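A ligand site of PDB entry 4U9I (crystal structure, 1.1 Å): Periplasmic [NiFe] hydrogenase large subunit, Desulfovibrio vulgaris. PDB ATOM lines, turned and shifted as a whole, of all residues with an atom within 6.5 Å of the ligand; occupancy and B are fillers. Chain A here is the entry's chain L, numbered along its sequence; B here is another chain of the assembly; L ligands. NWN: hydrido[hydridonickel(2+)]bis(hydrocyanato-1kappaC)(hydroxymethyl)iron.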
ATOM      1  N   GLU A  15     -18.692   8.755 -12.563  1.00  0.00           N
ATOM      2  CA  GLU A  15     -19.280   9.963 -13.107  1.00  0.00           C
ATOM      3  C   GLU A  15     -19.860  10.765 -11.937  1.00  0.00           C
ATOM      4  O   GLU A  15     -20.631  10.239 -11.121  1.00  0.00           O
ATOM      5  CB  GLU A  15     -20.360   9.637 -14.126  1.00  0.00           C
ATOM      6  CG  GLU A  15     -20.857  10.851 -14.919  1.00  0.00           C
ATOM      7  CD  GLU A  15     -21.579  11.868 -14.095  1.00  0.00           C
ATOM      8  OE1 GLU A  15     -21.370  13.149 -14.342  1.00  0.00           O
ATOM      9  OE2 GLU A  15     -22.334  11.510 -13.192  1.00  0.00           O
ATOM     10  N   THR A  61     -28.532  14.922 -18.849  1.00  0.00           N
ATOM     11  CA  THR A  61     -28.412  14.310 -17.515  1.00  0.00           C
ATOM     12  C   THR A  61     -27.009  13.681 -17.362  1.00  0.00           C
ATOM     13  O   THR A  61     -26.392  13.779 -16.297  1.00  0.00           O
ATOM     14  CB  THR A  61     -29.472  13.263 -17.277  1.00  0.00           C
ATOM     15  OG1 THR A  61     -30.764  13.867 -17.265  1.00  0.00           O
ATOM     16  CG2 THR A  61     -29.273  12.539 -15.954  1.00  0.00           C
ATOM     17  N   CYS A  62     -26.521  13.046 -18.416  1.00  0.00           N
ATOM     18  CA  CYS A  62     -25.285  12.290 -18.333  1.00  0.00           C
ATOM     19  C   CYS A  62     -24.694  12.053 -19.713  1.00  0.00           C
ATOM     20  O   CYS A  62     -25.394  11.567 -20.611  1.00  0.00           O
ATOM     21  CB  CYS A  62     -25.553  10.953 -17.638  1.00  0.00           C
ATOM     22  SG  CYS A  62     -24.050  10.020 -17.295  1.00  0.00           S
ATOM     23  N   GLY A  63     -23.387  12.292 -19.807  1.00  0.00           N
ATOM     24  CA  GLY A  63     -22.619  12.042 -21.020  1.00  0.00           C
ATOM     25  C   GLY A  63     -21.809  10.759 -20.948  1.00  0.00           C
ATOM     26  O   GLY A  63     -21.189  10.425 -21.978  1.00  0.00           O
ATOM     27  N   VAL A  64     -21.787  10.067 -19.805  1.00  0.00           N
ATOM     28  CA  VAL A  64     -21.195   8.732 -19.733  1.00  0.00           C
ATOM     29  C   VAL A  64     -22.228   7.770 -20.288  1.00  0.00           C
ATOM     30  O   VAL A  64     -22.022   7.114 -21.328  1.00  0.00           O
ATOM     31  CB  VAL A  64     -20.712   8.400 -18.308  1.00  0.00           C
ATOM     32  CG1 VAL A  64     -20.249   6.967 -18.239  1.00  0.00           C
ATOM     33  CG2 VAL A  64     -19.622   9.352 -17.902  1.00  0.00           C
ATOM     34  N   CYS A  65     -23.390   7.718 -19.640  1.00  0.00           N
ATOM     35  CA  CYS A  65     -24.562   7.022 -20.190  1.00  0.00           C
ATOM     36  C   CYS A  65     -25.305   7.953 -21.163  1.00  0.00           C
ATOM     37  O   CYS A  65     -26.509   8.163 -21.132  1.00  0.00           O
ATOM     38  CB  CYS A  65     -25.478   6.448 -19.105  1.00  0.00           C
ATOM     39  SG  CYS A  65     -26.273   7.662 -18.043  1.00  0.00           S
ATOM     40  N   THR A  66     -24.531   8.490 -22.107  1.00  0.00           N
ATOM     41  CA  THR A  66     -25.081   9.258 -23.212  1.00  0.00           C
ATOM     42  C   THR A  66     -26.091   8.386 -23.960  1.00  0.00           C
ATOM     43  O   THR A  66     -26.104   7.145 -23.824  1.00  0.00           O
ATOM     44  CB  THR A  66     -23.978   9.809 -24.097  1.00  0.00           C
ATOM     45  OG1 THR A  66     -24.543  10.776 -25.006  1.00  0.00           O
ATOM     46  CG2 THR A  66     -23.283   8.740 -24.925  1.00  0.00           C
ATOM     47  N   THR A  68     -28.867   7.217 -23.479  1.00  0.00           N
ATOM     48  CA  THR A  68     -29.887   6.515 -22.702  1.00  0.00           C
ATOM     49  C   THR A  68     -31.053   7.413 -22.307  1.00  0.00           C
ATOM     50  O   THR A  68     -32.219   6.970 -22.376  1.00  0.00           O
ATOM     51  CB  THR A  68     -29.292   5.847 -21.434  1.00  0.00           C
ATOM     52  OG1 THR A  68     -28.881   6.806 -20.468  1.00  0.00           O
ATOM     53  CG2 THR A  68     -28.172   4.856 -21.792  1.00  0.00           C
ATOM     54  N   HIS A  69     -30.812   8.629 -21.864  1.00  0.00           N
ATOM     55  CA  HIS A  69     -31.911   9.507 -21.450  1.00  0.00           C
ATOM     56  C   HIS A  69     -32.672  10.090 -22.662  1.00  0.00           C
ATOM     57  O   HIS A  69     -33.859  10.332 -22.570  1.00  0.00           O
ATOM     58  CB  HIS A  69     -31.381  10.642 -20.580  1.00  0.00           C
ATOM     59  CG  HIS A  69     -30.954  10.214 -19.234  1.00  0.00           C
ATOM     60  ND1 HIS A  69     -31.851  10.036 -18.197  1.00  0.00           N
ATOM     61  CD2 HIS A  69     -29.726   9.897 -18.763  1.00  0.00           C
ATOM     62  CE1 HIS A  69     -31.156   9.651 -17.147  1.00  0.00           C
ATOM     63  NE2 HIS A  69     -29.884   9.542 -17.447  1.00  0.00           N
ATOM     64  N   GLN A 100     -23.941   1.351 -26.992  1.00  0.00           N
ATOM     65  CA  GLN A 100     -23.689   2.094 -25.758  1.00  0.00           C
ATOM     66  C   GLN A 100     -23.278   1.170 -24.623  1.00  0.00           C
ATOM     67  O   GLN A 100     -22.328   1.477 -23.887  1.00  0.00           O
ATOM     68  CB  GLN A 100     -24.938   2.895 -25.365  1.00  0.00           C
ATOM     69  CG  GLN A 100     -24.851   3.548 -23.956  1.00  0.00           C
ATOM     70  CD  GLN A 100     -23.707   4.515 -23.781  1.00  0.00           C
ATOM     71  OE1 GLN A 100     -23.262   5.161 -24.753  1.00  0.00           O
ATOM     72  NE2 GLN A 100     -23.256   4.678 -22.552  1.00  0.00           N
ATOM     73  N   ASP A 104     -19.684   1.588 -22.684  1.00  0.00           N
ATOM     74  CA  ASP A 104     -19.770   1.994 -21.277  1.00  0.00           C
ATOM     75  C   ASP A 104     -19.083   0.947 -20.394  1.00  0.00           C
ATOM     76  O   ASP A 104     -18.232   1.263 -19.584  1.00  0.00           O
ATOM     77  CB  ASP A 104     -21.263   2.219 -20.968  1.00  0.00           C
ATOM     78  CG  ASP A 104     -21.540   3.101 -19.780  1.00  0.00           C
ATOM     79  OD1 ASP A 104     -20.697   3.122 -18.830  1.00  0.00           O
ATOM     80  OD2 ASP A 104     -22.649   3.708 -19.761  1.00  0.00           O
ATOM     81  N   VAL A 456     -36.066   2.378 -19.908  1.00  0.00           N
ATOM     82  CA  VAL A 456     -34.826   1.897 -20.517  1.00  0.00           C
ATOM     83  C   VAL A 456     -34.117   1.109 -19.413  1.00  0.00           C
ATOM     84  O   VAL A 456     -34.029   1.557 -18.282  1.00  0.00           O
ATOM     85  CB  VAL A 456     -33.950   3.071 -20.962  1.00  0.00           C
ATOM     86  CG1 VAL A 456     -32.569   2.622 -21.386  1.00  0.00           C
ATOM     87  CG2 VAL A 456     -34.618   3.843 -22.089  1.00  0.00           C
ATOM     88  N   ALA A 458     -30.629   0.746 -18.737  1.00  0.00           N
ATOM     89  CA  ALA A 458     -29.391   1.376 -19.115  1.00  0.00           C
ATOM     90  C   ALA A 458     -28.218   0.542 -18.539  1.00  0.00           C
ATOM     91  O   ALA A 458     -28.429  -0.427 -17.788  1.00  0.00           O
ATOM     92  CB  ALA A 458     -29.395   2.781 -18.552  1.00  0.00           C
ATOM     93  N   PRO A 459     -26.965   0.924 -18.874  1.00  0.00           N
ATOM     94  CA  PRO A 459     -25.831   0.161 -18.337  1.00  0.00           C
ATOM     95  C   PRO A 459     -25.795   0.078 -16.802  1.00  0.00           C
ATOM     96  O   PRO A 459     -25.192  -0.881 -16.291  1.00  0.00           O
ATOM     97  CB  PRO A 459     -24.621   0.887 -18.931  1.00  0.00           C
ATOM     98  CG  PRO A 459     -25.142   1.389 -20.259  1.00  0.00           C
ATOM     99  CD  PRO A 459     -26.529   1.890 -19.902  1.00  0.00           C
ATOM    100  N   ARG A 460     -26.392   1.034 -16.090  1.00  0.00           N
ATOM    101  CA  ARG A 460     -26.436   1.007 -14.640  1.00  0.00           C
ATOM    102  C   ARG A 460     -27.777   0.542 -14.102  1.00  0.00           C
ATOM    103  O   ARG A 460     -27.941   0.456 -12.861  1.00  0.00           O
ATOM    104  CB  ARG A 460     -26.026   2.362 -14.071  1.00  0.00           C
ATOM    105  CG  ARG A 460     -24.550   2.639 -14.383  1.00  0.00           C
ATOM    106  CD  ARG A 460     -24.217   4.158 -14.318  1.00  0.00           C
ATOM    107  NE  ARG A 460     -22.846   4.364 -14.743  1.00  0.00           N
ATOM    108  CZ  ARG A 460     -22.454   4.292 -16.029  1.00  0.00           C
ATOM    109  NH1 ARG A 460     -23.341   4.288 -17.018  1.00  0.00           N
ATOM    110  NH2 ARG A 460     -21.174   4.299 -16.327  1.00  0.00           N
ATOM    111  N   GLY A 461     -28.741   0.203 -14.973  1.00  0.00           N
ATOM    112  CA  GLY A 461     -30.008  -0.360 -14.537  1.00  0.00           C
ATOM    113  C   GLY A 461     -31.255   0.361 -14.987  1.00  0.00           C
ATOM    114  O   GLY A 461     -31.305   0.997 -16.016  1.00  0.00           O
ATOM    115  N   GLY A 462     -32.307   0.218 -14.195  1.00  0.00           N
ATOM    116  CA  GLY A 462     -33.649   0.642 -14.607  1.00  0.00           C
ATOM    117  C   GLY A 462     -33.859   2.132 -14.564  1.00  0.00           C
ATOM    118  O   GLY A 462     -33.913   2.734 -13.487  1.00  0.00           O
ATOM    119  N   LEU A 463     -34.002   2.722 -15.771  1.00  0.00           N
ATOM    120  CA  LEU A 463     -34.233   4.145 -15.986  1.00  0.00           C
ATOM    121  C   LEU A 463     -35.678   4.361 -16.402  1.00  0.00           C
ATOM    122  O   LEU A 463     -36.179   3.667 -17.299  1.00  0.00           O
ATOM    123  CB  LEU A 463     -33.304   4.632 -17.085  1.00  0.00           C
ATOM    124  CG  LEU A 463     -33.544   6.032 -17.610  1.00  0.00           C
ATOM    125  CD1 LEU A 463     -33.375   7.086 -16.533  1.00  0.00           C
ATOM    126  CD2 LEU A 463     -32.629   6.376 -18.792  1.00  0.00           C
ATOM    127  N   VAL A 480     -36.393   9.075 -12.804  1.00  0.00           N
ATOM    128  CA  VAL A 480     -35.998   8.163 -11.715  1.00  0.00           C
ATOM    129  C   VAL A 480     -34.897   7.283 -12.338  1.00  0.00           C
ATOM    130  O   VAL A 480     -35.175   6.533 -13.266  1.00  0.00           O
ATOM    131  CB  VAL A 480     -37.176   7.336 -11.187  1.00  0.00           C
ATOM    132  CG1 VAL A 480     -36.697   6.522  -9.937  1.00  0.00           C
ATOM    133  CG2 VAL A 480     -38.366   8.200 -10.882  1.00  0.00           C
ATOM    134  N   VAL A 481     -33.669   7.431 -11.877  1.00  0.00           N
ATOM    135  CA  VAL A 481     -32.519   6.991 -12.633  1.00  0.00           C
ATOM    136  C   VAL A 481     -31.852   5.815 -11.899  1.00  0.00           C
ATOM    137  O   VAL A 481     -31.997   5.697 -10.672  1.00  0.00           O
ATOM    138  CB  VAL A 481     -31.638   8.238 -12.908  1.00  0.00           C
ATOM    139  CG1 VAL A 481     -30.466   7.949 -13.830  1.00  0.00           C
ATOM    140  CG2 VAL A 481     -32.500   9.342 -13.489  1.00  0.00           C
ATOM    141  N   PRO A 482     -31.136   4.931 -12.615  1.00  0.00           N
ATOM    142  CA  PRO A 482     -30.608   3.748 -11.903  1.00  0.00           C
ATOM    143  C   PRO A 482     -29.757   4.058 -10.680  1.00  0.00           C
ATOM    144  O   PRO A 482     -29.950   3.487  -9.610  1.00  0.00           O
ATOM    145  CB  PRO A 482     -29.808   2.990 -13.003  1.00  0.00           C
ATOM    146  CG  PRO A 482     -30.208   3.612 -14.303  1.00  0.00           C
ATOM    147  CD  PRO A 482     -31.049   4.754 -14.083  1.00  0.00           C
ATOM    148  N   SER A 483     -28.847   5.029 -10.805  1.00  0.00           N
ATOM    149  CA  SER A 483     -28.017   5.391  -9.667  1.00  0.00           C
ATOM    150  C   SER A 483     -28.805   6.025  -8.556  1.00  0.00           C
ATOM    151  O   SER A 483     -28.343   6.011  -7.412  1.00  0.00           O
ATOM    152  CB  SER A 483     -26.866   6.321 -10.075  1.00  0.00           C
ATOM    153  OG  SER A 483     -25.888   5.650 -10.870  1.00  0.00           O
ATOM    154  N   THR A 484     -29.980   6.596  -8.862  1.00  0.00           N
ATOM    155  CA  THR A 484     -30.856   7.079  -7.776  1.00  0.00           C
ATOM    156  C   THR A 484     -31.261   5.883  -6.886  1.00  0.00           C
ATOM    157  O   THR A 484     -31.221   5.947  -5.659  1.00  0.00           O
ATOM    158  CB  THR A 484     -32.146   7.774  -8.306  1.00  0.00           C
ATOM    159  OG1 THR A 484     -31.857   8.561  -9.478  1.00  0.00           O
ATOM    160  CG2 THR A 484     -32.726   8.662  -7.240  1.00  0.00           C
ATOM    161  N   ASP A 525     -20.829   1.070 -10.284  1.00  0.00           N
ATOM    162  CA  ASP A 525     -20.681   2.005 -11.417  1.00  0.00           C
ATOM    163  C   ASP A 525     -21.514   3.268 -11.179  1.00  0.00           C
ATOM    164  O   ASP A 525     -22.424   3.584 -11.947  1.00  0.00           O
ATOM    165  CB  ASP A 525     -21.044   1.244 -12.696  1.00  0.00           C
ATOM    166  CG  ASP A 525     -20.801   1.992 -14.005  1.00  0.00           C
ATOM    167  OD1 ASP A 525     -20.157   3.074 -14.004  1.00  0.00           O
ATOM    168  OD2 ASP A 525     -21.278   1.419 -15.026  1.00  0.00           O
ATOM    169  N   PRO A 526     -21.206   4.014 -10.123  1.00  0.00           N
ATOM    170  CA  PRO A 526     -22.011   5.186  -9.788  1.00  0.00           C
ATOM    171  C   PRO A 526     -22.004   6.270 -10.881  1.00  0.00           C
ATOM    172  O   PRO A 526     -20.960   6.572 -11.465  1.00  0.00           O
ATOM    173  CB  PRO A 526     -21.331   5.743  -8.533  1.00  0.00           C
ATOM    174  CG  PRO A 526     -20.610   4.552  -7.939  1.00  0.00           C
ATOM    175  CD  PRO A 526     -20.093   3.831  -9.174  1.00  0.00           C
ATOM    176  N   CYS A 527     -23.165   6.916 -11.036  1.00  0.00           N
ATOM    177  CA  CYS A 527     -23.341   8.010 -11.895  1.00  0.00           C
ATOM    178  C   CYS A 527     -24.143   9.070 -11.264  1.00  0.00           C
ATOM    179  O   CYS A 527     -25.367   8.929 -11.144  1.00  0.00           O
ATOM    180  CB  CYS A 527     -23.912   7.521 -13.270  1.00  0.00           C
ATOM    181  SG  CYS A 527     -23.805   8.738 -14.578  1.00  0.00           S
ATOM    182  N   ILE A 528     -23.494  10.083 -10.706  1.00  0.00           N
ATOM    183  CA  ILE A 528     -24.142  11.010  -9.783  1.00  0.00           C
ATOM    184  C   ILE A 528     -24.921  12.093 -10.536  1.00  0.00           C
ATOM    185  O   ILE A 528     -25.969  12.567 -10.022  1.00  0.00           O
ATOM    186  CB  ILE A 528     -23.162  11.623  -8.782  1.00  0.00           C
ATOM    187  CG1 ILE A 528     -22.258  10.553  -8.167  1.00  0.00           C
ATOM    188  CG2 ILE A 528     -23.928  12.392  -7.665  1.00  0.00           C
ATOM    189  CD1 ILE A 528     -22.967   9.388  -7.506  1.00  0.00           C
ATOM    190  N   ALA A 529     -24.464  12.511 -11.699  1.00  0.00           N
ATOM    191  CA  ALA A 529     -25.254  13.418 -12.519  1.00  0.00           C
ATOM    192  C   ALA A 529     -26.569  12.728 -12.911  1.00  0.00           C
ATOM    193  O   ALA A 529     -27.640  13.339 -12.853  1.00  0.00           O
ATOM    194  CB  ALA A 529     -24.449  13.842 -13.769  1.00  0.00           C
ATOM    195  N   CYS A 530     -26.492  11.444 -13.241  1.00  0.00           N
ATOM    196  CA  CYS A 530     -27.676  10.611 -13.404  1.00  0.00           C
ATOM    197  C   CYS A 530     -28.535  10.592 -12.156  1.00  0.00           C
ATOM    198  O   CYS A 530     -29.753  10.814 -12.220  1.00  0.00           O
ATOM    199  CB  CYS A 530     -27.286   9.186 -13.792  1.00  0.00           C
ATOM    200  SG  CYS A 530     -27.325   8.902 -15.562  1.00  0.00           S
ATOM    201  N   GLY A 531     -27.928  10.248 -11.033  1.00  0.00           N
ATOM    202  CA  GLY A 531     -28.751  10.023  -9.857  1.00  0.00           C
ATOM    203  C   GLY A 531     -29.525  11.233  -9.378  1.00  0.00           C
ATOM    204  O   GLY A 531     -30.637  11.074  -8.894  1.00  0.00           O
ATOM    205  N   CYS B  15     -22.182  17.058 -16.960  1.00  0.00           N
ATOM    206  CA  CYS B  15     -22.725  15.732 -17.222  1.00  0.00           C
ATOM    207  C   CYS B  15     -21.627  14.725 -17.572  1.00  0.00           C
ATOM    208  O   CYS B  15     -21.920  13.543 -17.777  1.00  0.00           O
ATOM    209  CB  CYS B  15     -23.777  15.761 -18.324  1.00  0.00           C
ATOM    210  SG  CYS B  15     -23.096  15.810 -20.022  1.00  0.00           S
HETATM  211 FE   NWN L   1     -27.024   6.681 -16.141  1.00  0.00          FE
HETATM  212 NI   NWN L   1     -24.992   8.241 -16.326  1.00  0.00          NI
HETATM  213  C1  NWN L   1     -27.229   6.148 -14.365  1.00  0.00           C
HETATM  214  N1  NWN L   1     -27.296   5.825 -13.270  1.00  0.00           N
HETATM  215  C2  NWN L   1     -26.640   4.910 -16.702  1.00  0.00           C
HETATM  216  N2  NWN L   1     -26.436   3.806 -17.101  1.00  0.00           N
HETATM  217  C3  NWN L   1     -28.678   6.346 -16.543  1.00  0.00           C
HETATM  218  O3  NWN L   1     -29.785   6.102 -16.833  1.00  0.00           O
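The side-chain hydroxyl (OG) of Ser 483 lies within hydrogen-bond range of the backbone NH (N) of Cys 527 (3.0 Å).
SG of Cys 527 sits close to OE2 of Glu 15 of chain A (3.4 Å).
The backbone carbonyl oxygen (O) of Cys 65 lies within hydrogen-bond range of the side-chain hydroxyl (OG1) of Thr 68.
The side-chain sulfur of Cys 530 sits close to a ring nitrogen (NE2) of His 69, at 3.2 Å.
The guanidinium group (NH2) of Arg 460 is in salt-bridge range of the side-chain carboxylate (OD1) of Asp 104 (2.8 Å).
The guanidinium group (NH2) of Arg 460 lies within salt-bridge range of the side-chain carboxylate (OD1) of Asp 525 (2.8 Å).
The backbone carbonyl oxygen of Val 456 sits at hydrogen-bond distance from the backbone NH of Leu 463 (2.8 Å).
O of Val 481 is in hydrogen-bond range of OG1 of Thr 484 (3.1 Å).
A nickel atom (NI) of the ligand is bound by the side-chain sulfur (SG) of Cys 527 (2.2 Å).
A nickel atom (NI) of the ligand is bound by the side-chain sulfur (SG) of Cys 65 (2.2 Å).
The side-chain sulfur (SG) of Cys 62 binds a nickel atom (NI) of the ligand (2.2 Å).
SG of Cys 530 is bound to FE of the ligand (2.3 Å).
The backbone NH of Ser 483 is in hydrogen-bond range of a nitrogen (N1) of the ligand, at 3.0 Å.
N1 of the ligand lies within hydrogen-bond range of OG of Ser 483, at 2.8 Å.
N of Arg 460 sits at hydrogen-bond distance from N2 of the ligand, 3.0 Å away.
A nitrogen (N2) of the ligand sits at hydrogen-bond distance from the guanidinium group of Arg 460 (3.1 Å).
A ring nitrogen (NE2) of His 69 is in hydrogen-bond range of an oxygen (O3) of the ligand (3.5 Å).
The backbone nitrogen (N) of Pro 459 lies close to a nitrogen (N2) of the ligand.
Thr 68 touches the ligand.
Ala 458 touches the ligand (CB to N2, 3.5 Å).
Leu 463 touches the ligand.
Val 481 touches the ligand.
Pro 482 touches the ligand (CD to O3, 3.3 Å).
Hydrophobic or aromatic side chains that line the ligand: His 69, Ala 458, Pro 459, Leu 463, Val 481 and Pro 482.
Of the 31 residues printed, 13 come within 4 Å of the ligand.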
